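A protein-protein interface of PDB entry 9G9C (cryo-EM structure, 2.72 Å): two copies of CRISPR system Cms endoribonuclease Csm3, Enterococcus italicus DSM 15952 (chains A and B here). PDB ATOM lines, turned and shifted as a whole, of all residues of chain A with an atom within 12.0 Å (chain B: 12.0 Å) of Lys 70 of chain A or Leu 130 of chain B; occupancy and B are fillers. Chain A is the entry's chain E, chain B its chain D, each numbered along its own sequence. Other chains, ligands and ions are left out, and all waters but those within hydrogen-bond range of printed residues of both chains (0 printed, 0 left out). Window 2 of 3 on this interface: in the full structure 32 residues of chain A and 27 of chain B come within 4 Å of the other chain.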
ATOM      1  N   ARG A  56      12.936  11.936  13.228  1.00  0.00           N
ATOM      2  CA  ARG A  56      12.779  10.623  12.616  1.00  0.00           C
ATOM      3  C   ARG A  56      11.427  10.487  11.930  1.00  0.00           C
ATOM      4  O   ARG A  56      11.341   9.930  10.832  1.00  0.00           O
ATOM      5  CB  ARG A  56      12.963   9.527  13.664  1.00  0.00           C
ATOM      6  CG  ARG A  56      12.751   8.126  13.119  1.00  0.00           C
ATOM      7  CD  ARG A  56      13.283   7.064  14.059  1.00  0.00           C
ATOM      8  NE  ARG A  56      13.043   5.722  13.542  1.00  0.00           N
ATOM      9  CZ  ARG A  56      13.626   4.625  14.005  1.00  0.00           C
ATOM     10  NH1 ARG A  56      14.497   4.672  14.997  1.00  0.00           N
ATOM     11  NH2 ARG A  56      13.329   3.451  13.455  1.00  0.00           N
ATOM     12  N   SER A  57      10.360  10.991  12.556  1.00  0.00           N
ATOM     13  CA  SER A  57       9.041  10.919  11.937  1.00  0.00           C
ATOM     14  C   SER A  57       8.992  11.718  10.643  1.00  0.00           C
ATOM     15  O   SER A  57       8.465  11.243   9.628  1.00  0.00           O
ATOM     16  CB  SER A  57       7.978  11.419  12.914  1.00  0.00           C
ATOM     17  OG  SER A  57       6.717  11.527  12.282  1.00  0.00           O
ATOM     18  N   ALA A  60      11.040   9.952   7.977  1.00  0.00           N
ATOM     19  CA  ALA A  60      10.328   8.776   7.491  1.00  0.00           C
ATOM     20  C   ALA A  60       9.196   9.162   6.551  1.00  0.00           C
ATOM     21  O   ALA A  60       8.958   8.483   5.546  1.00  0.00           O
ATOM     22  CB  ALA A  60       9.797   7.963   8.669  1.00  0.00           C
ATOM     23  N   LYS A  61       8.478  10.242   6.864  1.00  0.00           N
ATOM     24  CA  LYS A  61       7.429  10.702   5.960  1.00  0.00           C
ATOM     25  C   LYS A  61       8.014  11.205   4.645  1.00  0.00           C
ATOM     26  O   LYS A  61       7.418  11.009   3.580  1.00  0.00           O
ATOM     27  CB  LYS A  61       6.594  11.790   6.634  1.00  0.00           C
ATOM     28  CG  LYS A  61       5.281  11.289   7.207  1.00  0.00           C
ATOM     29  CD  LYS A  61       4.948  11.971   8.522  1.00  0.00           C
ATOM     30  CE  LYS A  61       4.942  13.481   8.376  1.00  0.00           C
ATOM     31  NZ  LYS A  61       5.166  14.159   9.681  1.00  0.00           N
ATOM     32  N   GLY A  64       9.394   8.067   2.812  1.00  0.00           N
ATOM     33  CA  GLY A  64       8.260   7.241   2.460  1.00  0.00           C
ATOM     34  C   GLY A  64       8.004   6.141   3.466  1.00  0.00           C
ATOM     35  O   GLY A  64       8.935   5.644   4.107  1.00  0.00           O
ATOM     36  N   LEU A  65       6.742   5.758   3.617  1.00  0.00           N
ATOM     37  CA  LEU A  65       6.341   4.692   4.524  1.00  0.00           C
ATOM     38  C   LEU A  65       5.786   3.533   3.709  1.00  0.00           C
ATOM     39  O   LEU A  65       4.985   3.744   2.792  1.00  0.00           O
ATOM     40  CB  LEU A  65       5.292   5.186   5.523  1.00  0.00           C
ATOM     41  CG  LEU A  65       5.679   6.360   6.424  1.00  0.00           C
ATOM     42  CD1 LEU A  65       4.457   6.895   7.148  1.00  0.00           C
ATOM     43  CD2 LEU A  65       6.750   5.947   7.418  1.00  0.00           C
ATOM     44  N   ILE A  66       6.216   2.319   4.037  1.00  0.00           N
ATOM     45  CA  ILE A  66       5.686   1.125   3.387  1.00  0.00           C
ATOM     46  C   ILE A  66       4.221   0.998   3.786  1.00  0.00           C
ATOM     47  O   ILE A  66       3.849   1.402   4.897  1.00  0.00           O
ATOM     48  CB  ILE A  66       6.491  -0.129   3.763  1.00  0.00           C
ATOM     49  CG1 ILE A  66       6.517  -0.322   5.278  1.00  0.00           C
ATOM     50  CG2 ILE A  66       7.906  -0.035   3.217  1.00  0.00           C
ATOM     51  CD1 ILE A  66       7.197  -1.600   5.719  1.00  0.00           C
ATOM     52  N   PRO A  67       3.355   0.479   2.917  1.00  0.00           N
ATOM     53  CA  PRO A  67       1.933   0.374   3.268  1.00  0.00           C
ATOM     54  C   PRO A  67       1.729  -0.489   4.504  1.00  0.00           C
ATOM     55  O   PRO A  67       2.276  -1.589   4.613  1.00  0.00           O
ATOM     56  CB  PRO A  67       1.308  -0.262   2.021  1.00  0.00           C
ATOM     57  CG  PRO A  67       2.248   0.081   0.913  1.00  0.00           C
ATOM     58  CD  PRO A  67       3.614   0.062   1.528  1.00  0.00           C
ATOM     59  N   GLY A  68       0.931   0.021   5.436  1.00  0.00           N
ATOM     60  CA  GLY A  68       0.672  -0.684   6.678  1.00  0.00           C
ATOM     61  C   GLY A  68       1.887  -0.867   7.561  1.00  0.00           C
ATOM     62  O   GLY A  68       2.081  -1.952   8.124  1.00  0.00           O
ATOM     63  N   GLN A  69       2.715   0.166   7.697  1.00  0.00           N
ATOM     64  CA  GLN A  69       3.896   0.091   8.550  1.00  0.00           C
ATOM     65  C   GLN A  69       3.459   0.217  10.004  1.00  0.00           C
ATOM     66  O   GLN A  69       2.944   1.260  10.417  1.00  0.00           O
ATOM     67  CB  GLN A  69       4.900   1.177   8.181  1.00  0.00           C
ATOM     68  CG  GLN A  69       6.082   1.251   9.126  1.00  0.00           C
ATOM     69  CD  GLN A  69       7.139   2.227   8.666  1.00  0.00           C
ATOM     70  OE1 GLN A  69       7.174   2.618   7.501  1.00  0.00           O
ATOM     71  NE2 GLN A  69       8.011   2.628   9.582  1.00  0.00           N
ATOM     72  N   LYS A  70       3.669  -0.842  10.782  1.00  0.00           N
ATOM     73  CA  LYS A  70       3.214  -0.873  12.165  1.00  0.00           C
ATOM     74  C   LYS A  70       4.283  -0.438  13.154  1.00  0.00           C
ATOM     75  O   LYS A  70       3.955   0.178  14.174  1.00  0.00           O
ATOM     76  CB  LYS A  70       2.736  -2.282  12.529  1.00  0.00           C
ATOM     77  CG  LYS A  70       1.878  -2.943  11.464  1.00  0.00           C
ATOM     78  CD  LYS A  70       1.085  -4.104  12.040  1.00  0.00           C
ATOM     79  CE  LYS A  70      -0.282  -4.225  11.387  1.00  0.00           C
ATOM     80  NZ  LYS A  70      -1.383  -4.019  12.367  1.00  0.00           N
ATOM     81  N   MET A  71       5.549  -0.736  12.881  1.00  0.00           N
ATOM     82  CA  MET A  71       6.629  -0.490  13.820  1.00  0.00           C
ATOM     83  C   MET A  71       7.619   0.516  13.247  1.00  0.00           C
ATOM     84  O   MET A  71       7.608   0.827  12.054  1.00  0.00           O
ATOM     85  CB  MET A  71       7.362  -1.790  14.178  1.00  0.00           C
ATOM     86  CG  MET A  71       6.453  -2.926  14.616  1.00  0.00           C
ATOM     87  SD  MET A  71       5.161  -2.401  15.759  1.00  0.00           S
ATOM     88  CE  MET A  71       5.175  -3.753  16.932  1.00  0.00           C
ATOM     89  N   HIS A  72       8.477   1.029  14.128  1.00  0.00           N
ATOM     90  CA  HIS A  72       9.521   1.962  13.733  1.00  0.00           C
ATOM     91  C   HIS A  72      10.736   1.273  13.130  1.00  0.00           C
ATOM     92  O   HIS A  72      11.570   1.951  12.519  1.00  0.00           O
ATOM     93  CB  HIS A  72       9.954   2.804  14.935  1.00  0.00           C
ATOM     94  CG  HIS A  72       8.889   3.730  15.434  1.00  0.00           C
ATOM     95  ND1 HIS A  72       8.894   5.081  15.167  1.00  0.00           N
ATOM     96  CD2 HIS A  72       7.784   3.497  16.178  1.00  0.00           C
ATOM     97  CE1 HIS A  72       7.838   5.641  15.728  1.00  0.00           C
ATOM     98  NE2 HIS A  72       7.148   4.703  16.347  1.00  0.00           N
ATOM     99  N   ASN A  73      10.861  -0.043  13.286  1.00  0.00           N
ATOM    100  CA  ASN A  73      11.954  -0.787  12.673  1.00  0.00           C
ATOM    101  C   ASN A  73      11.694  -1.108  11.210  1.00  0.00           C
ATOM    102  O   ASN A  73      12.578  -1.659  10.547  1.00  0.00           O
ATOM    103  CB  ASN A  73      12.217  -2.079  13.449  1.00  0.00           C
ATOM    104  CG  ASN A  73      12.635  -1.822  14.878  1.00  0.00           C
ATOM    105  OD1 ASN A  73      12.306  -2.588  15.782  1.00  0.00           O
ATOM    106  ND2 ASN A  73      13.360  -0.732  15.093  1.00  0.00           N
ATOM    107  N   GLN A  74      10.511  -0.784  10.697  1.00  0.00           N
ATOM    108  CA  GLN A  74      10.184  -0.972   9.292  1.00  0.00           C
ATOM    109  C   GLN A  74      10.509   0.250   8.445  1.00  0.00           C
ATOM    110  O   GLN A  74      10.189   0.261   7.253  1.00  0.00           O
ATOM    111  CB  GLN A  74       8.702  -1.326   9.138  1.00  0.00           C
ATOM    112  CG  GLN A  74       8.319  -2.674   9.715  1.00  0.00           C
ATOM    113  CD  GLN A  74       6.829  -2.927   9.644  1.00  0.00           C
ATOM    114  OE1 GLN A  74       6.027  -2.052   9.960  1.00  0.00           O
ATOM    115  NE2 GLN A  74       6.451  -4.127   9.222  1.00  0.00           N
ATOM    116  N   ASP A  75      11.126   1.274   9.029  1.00  0.00           N
ATOM    117  CA  ASP A  75      11.496   2.468   8.288  1.00  0.00           C
ATOM    118  C   ASP A  75      12.572   2.138   7.254  1.00  0.00           C
ATOM    119  O   ASP A  75      13.056   1.007   7.154  1.00  0.00           O
ATOM    120  CB  ASP A  75      11.979   3.560   9.242  1.00  0.00           C
ATOM    121  CG  ASP A  75      10.860   4.131  10.090  1.00  0.00           C
ATOM    122  OD1 ASP A  75       9.718   4.213   9.593  1.00  0.00           O
ATOM    123  OD2 ASP A  75      11.122   4.501  11.252  1.00  0.00           O
ATOM    124  N   ALA A  76      12.951   3.147   6.477  1.00  0.00           N
ATOM    125  CA  ALA A  76      13.948   2.954   5.439  1.00  0.00           C
ATOM    126  C   ALA A  76      15.296   2.595   6.063  1.00  0.00           C
ATOM    127  O   ALA A  76      15.570   2.948   7.214  1.00  0.00           O
ATOM    128  CB  ALA A  76      14.083   4.215   4.589  1.00  0.00           C
ATOM    129  N   LEU A  80      16.950   3.682   9.775  1.00  0.00           N
ATOM    130  CA  LEU A  80      17.434   2.724  10.764  1.00  0.00           C
ATOM    131  C   LEU A  80      18.931   2.872  10.994  1.00  0.00           C
ATOM    132  O   LEU A  80      19.419   2.620  12.100  1.00  0.00           O
ATOM    133  CB  LEU A  80      17.102   1.300  10.323  1.00  0.00           C
ATOM    134  CG  LEU A  80      15.652   1.034   9.917  1.00  0.00           C
ATOM    135  CD1 LEU A  80      15.479  -0.407   9.474  1.00  0.00           C
ATOM    136  CD2 LEU A  80      14.706   1.364  11.057  1.00  0.00           C
ATOM    137  N   SER A  86      15.958  -2.014  16.011  1.00  0.00           N
ATOM    138  CA  SER A  86      15.736  -2.939  17.114  1.00  0.00           C
ATOM    139  C   SER A  86      15.304  -4.327  16.654  1.00  0.00           C
ATOM    140  O   SER A  86      14.855  -5.122  17.489  1.00  0.00           O
ATOM    141  CB  SER A  86      14.691  -2.370  18.079  1.00  0.00           C
ATOM    142  OG  SER A  86      14.697  -3.073  19.305  1.00  0.00           O
ATOM    143  N   GLN A  87      15.420  -4.643  15.367  1.00  0.00           N
ATOM    144  CA  GLN A  87      14.967  -5.932  14.865  1.00  0.00           C
ATOM    145  C   GLN A  87      15.775  -7.070  15.479  1.00  0.00           C
ATOM    146  O   GLN A  87      16.931  -6.900  15.874  1.00  0.00           O
ATOM    147  CB  GLN A  87      15.081  -5.979  13.340  1.00  0.00           C
ATOM    148  CG  GLN A  87      13.923  -5.332  12.605  1.00  0.00           C
ATOM    149  CD  GLN A  87      12.686  -6.208  12.577  1.00  0.00           C
ATOM    150  OE1 GLN A  87      12.744  -7.392  12.903  1.00  0.00           O
ATOM    151  NE2 GLN A  87      11.558  -5.627  12.186  1.00  0.00           N
ATOM    152  N   THR B 126       5.327   7.070  22.620  1.00  0.00           N
ATOM    153  CA  THR B 126       5.650   6.654  21.262  1.00  0.00           C
ATOM    154  C   THR B 126       4.405   6.794  20.397  1.00  0.00           C
ATOM    155  O   THR B 126       3.298   6.478  20.840  1.00  0.00           O
ATOM    156  CB  THR B 126       6.206   5.220  21.228  1.00  0.00           C
ATOM    157  OG1 THR B 126       6.935   5.017  20.010  1.00  0.00           O
ATOM    158  CG2 THR B 126       5.107   4.172  21.341  1.00  0.00           C
ATOM    159  N   ILE B 127       4.577   7.314  19.188  1.00  0.00           N
ATOM    160  CA  ILE B 127       3.478   7.469  18.243  1.00  0.00           C
ATOM    161  C   ILE B 127       3.619   6.391  17.181  1.00  0.00           C
ATOM    162  O   ILE B 127       4.654   6.300  16.509  1.00  0.00           O
ATOM    163  CB  ILE B 127       3.456   8.873  17.616  1.00  0.00           C
ATOM    164  CG1 ILE B 127       3.009   9.924  18.635  1.00  0.00           C
ATOM    165  CG2 ILE B 127       2.532   8.900  16.413  1.00  0.00           C
ATOM    166  CD1 ILE B 127       4.118  10.475  19.493  1.00  0.00           C
ATOM    167  N   SER B 128       2.583   5.571  17.030  1.00  0.00           N
ATOM    168  CA  SER B 128       2.633   4.467  16.085  1.00  0.00           C
ATOM    169  C   SER B 128       2.647   4.979  14.651  1.00  0.00           C
ATOM    170  O   SER B 128       1.999   5.976  14.323  1.00  0.00           O
ATOM    171  CB  SER B 128       1.442   3.535  16.300  1.00  0.00           C
ATOM    172  OG  SER B 128       0.222   4.246  16.213  1.00  0.00           O
ATOM    173  N   ARG B 129       3.399   4.288  13.794  1.00  0.00           N
ATOM    174  CA  ARG B 129       3.436   4.613  12.374  1.00  0.00           C
ATOM    175  C   ARG B 129       2.178   4.182  11.638  1.00  0.00           C
ATOM    176  O   ARG B 129       2.002   4.554  10.473  1.00  0.00           O
ATOM    177  CB  ARG B 129       4.654   3.963  11.714  1.00  0.00           C
ATOM    178  CG  ARG B 129       5.992   4.465  12.219  1.00  0.00           C
ATOM    179  CD  ARG B 129       6.505   5.623  11.383  1.00  0.00           C
ATOM    180  NE  ARG B 129       7.902   5.915  11.681  1.00  0.00           N
ATOM    181  CZ  ARG B 129       8.308   6.818  12.563  1.00  0.00           C
ATOM    182  NH1 ARG B 129       7.445   7.561  13.236  1.00  0.00           N
ATOM    183  NH2 ARG B 129       9.609   6.976  12.777  1.00  0.00           N
ATOM    184  N   LEU B 130       1.306   3.409  12.283  1.00  0.00           N
ATOM    185  CA  LEU B 130       0.087   2.905  11.664  1.00  0.00           C
ATOM    186  C   LEU B 130      -1.151   3.690  12.080  1.00  0.00           C
ATOM    187  O   LEU B 130      -1.876   4.203  11.224  1.00  0.00           O
ATOM    188  CB  LEU B 130      -0.098   1.425  12.014  1.00  0.00           C
ATOM    189  CG  LEU B 130      -1.191   0.682  11.249  1.00  0.00           C
ATOM    190  CD1 LEU B 130      -0.873   0.645   9.765  1.00  0.00           C
ATOM    191  CD2 LEU B 130      -1.363  -0.718  11.800  1.00  0.00           C
ATOM    192  N   THR B 131      -1.402   3.798  13.383  1.00  0.00           N
ATOM    193  CA  THR B 131      -2.617   4.414  13.891  1.00  0.00           C
ATOM    194  C   THR B 131      -2.411   5.819  14.435  1.00  0.00           C
ATOM    195  O   THR B 131      -3.397   6.472  14.792  1.00  0.00           O
ATOM    196  CB  THR B 131      -3.233   3.537  14.992  1.00  0.00           C
ATOM    197  OG1 THR B 131      -2.277   3.342  16.041  1.00  0.00           O
ATOM    198  CG2 THR B 131      -3.644   2.188  14.432  1.00  0.00           C
ATOM    199  N   ALA B 132      -1.166   6.295  14.514  1.00  0.00           N
ATOM    200  CA  ALA B 132      -0.845   7.609  15.072  1.00  0.00           C
ATOM    201  C   ALA B 132      -1.345   7.750  16.505  1.00  0.00           C
ATOM    202  O   ALA B 132      -1.683   8.848  16.951  1.00  0.00           O
ATOM    203  CB  ALA B 132      -1.396   8.741  14.200  1.00  0.00           C
ATOM    204  N   VAL B 133      -1.387   6.641  17.237  1.00  0.00           N
ATOM    205  CA  VAL B 133      -1.871   6.615  18.611  1.00  0.00           C
ATOM    206  C   VAL B 133      -0.668   6.666  19.539  1.00  0.00           C
ATOM    207  O   VAL B 133       0.251   5.847  19.424  1.00  0.00           O
ATOM    208  CB  VAL B 133      -2.725   5.366  18.884  1.00  0.00           C
ATOM    209  CG1 VAL B 133      -3.060   5.268  20.365  1.00  0.00           C
ATOM    210  CG2 VAL B 133      -3.992   5.399  18.052  1.00  0.00           C
ATOM    211  N   ALA B 134      -0.667   7.629  20.453  1.00  0.00           N
ATOM    212  CA  ALA B 134       0.419   7.755  21.409  1.00  0.00           C
ATOM    213  C   ALA B 134       0.257   6.749  22.540  1.00  0.00           C
ATOM    214  O   ALA B 134      -0.844   6.537  23.055  1.00  0.00           O
ATOM    215  CB  ALA B 134       0.477   9.174  21.973  1.00  0.00           C
ATOM    216  N   ASN B 135       1.388   6.186  22.979  1.00  0.00           N
ATOM    217  CA  ASN B 135       1.377   5.236  24.123  1.00  0.00           C
ATOM    218  C   ASN B 135       2.310   5.772  25.206  1.00  0.00           C
ATOM    219  O   ASN B 135       3.538   5.715  25.004  1.00  0.00           O
ATOM    220  CB  ASN B 135       1.817   3.839  23.719  1.00  0.00           C
ATOM    221  CG  ASN B 135       1.883   2.899  24.900  1.00  0.00           C
ATOM    222  OD1 ASN B 135       2.940   2.325  25.177  1.00  0.00           O
ATOM    223  ND2 ASN B 135       0.771   2.724  25.598  1.00  0.00           N
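O of His 72 of chain A is in hydrogen-bond range of NH2 of Arg 56 of chain A (2.5 Å).
The guanidinium group (NE) of Arg 56 of chain A is in salt-bridge range of the side-chain carboxylate (OD2) of Asp 75 of chain A (3.2 Å).
The side-chain amide nitrogen (NE2) of Gln 69 of chain A sits at hydrogen-bond distance from the backbone carbonyl oxygen (O) of Met 71 of chain A.
The backbone NH (N) of Lys 70 of chain A is in hydrogen-bond range of the side-chain amide oxygen (OE1) of Gln 74 of chain A.
OE1 of Gln 74 of chain A lies within hydrogen-bond range of N of Met 71 of chain A (3.2 Å).
O of Thr 126 of chain B sits at hydrogen-bond distance from N of Asn 135 of chain B (2.9 Å).
NH2 of Arg 129 of chain B touches CG of Arg 56 of chain A, at 3.4 Å.
Ser 57 of chain A touches Arg 129 of chain B (CB to NH1, 3.9 Å).
Arg 129 of chain B touches Leu 65 of chain A (CD to CD2, 3.99 Å).
Gly 68 of chain A touches Leu 130 of chain B.
Lys 70 of chain A touches Leu 130 of chain B (NZ to CD2, 3.3 Å).
Arg 129 of chain B touches Met 71 of chain A (CG to O, 3.98 Å).
NE2 of His 72 of chain A touches OG1 of Thr 126 of chain B, 3.7 Å away.
The backbone carbonyl oxygen (O) of Gln 69 of chain A is in hydrogen-bond range of the backbone NH (N) of Leu 130 of chain B, at 3.3 Å.
The backbone carbonyl oxygen (O) of Ile 127 of chain B lies within hydrogen-bond range of a ring nitrogen (NE2) of His 72 of chain A (3.0 Å).
ND1 of His 72 of chain A sits at hydrogen-bond distance from NH2 of Arg 129 of chain B.
OD1 of Asp 75 of chain A lies within salt-bridge range of NE of Arg 129 of chain B (3.2 Å).
O of Arg 129 of chain B sits close to O of Gln 69 of chain A (3.4 Å).
Of the 20 printed residues of chain A, 9 touch a printed residue of chain B.
Hydrophobic or aromatic side chains of chain A within 4 Å of the printed part of chain B: Leu 65 and His 72.
Hydrophobic or aromatic side chains of chain B that line the printed part of chain A: Leu 130.
Among the printed residues, Asp or Glu carboxylates within 4 Å of a Lys or Arg side-chain nitrogen of the other chain: Asp 75 of chain A with Arg 129 of chain B (3.2 Å).
Of the printed residues of chain B, Arg 56 of chain A touches Arg 129.
Of chain B, only Leu 130 comes within 4 Å of Gly 68 of chain A.
Of chain B, only Leu 130 (3.3 Å) comes within 4 Å of Lys 70 of chain A.
Of chain B, only Thr 126 (3.7 Å), Ile 127 (3.0 Å) and Arg 129 (3.1 Å) come within 4 Å of His 72 of chain A.
No residue of chain B comes within 4 Å of Gln 74 of chain A.
Of the printed residues of chain B, Asp 75 of chain A touches Arg 129.
No residue of chain A comes within 4 Å of Ser 128 of chain B.
Leu 130 of chain B touches three residues of chain A.
No residue of chain A comes within 4 Å of Thr 131 of chain B.
No residue of chain A comes within 4 Å of Ala 132 of chain B.
Ala 134 of chain B touches none of the printed residues of chain A.
Asn 135 of chain B touches none of the printed residues of chain A.
The nearest printed residue of chain B that does not touch Arg 56 of chain A is Ile 127 of chain B (8.9 Å).
No position is printed for both chains.
Of the 12 pairs that touch across the chains among the printed residues, none has its exchanged pair printed and touching as well.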
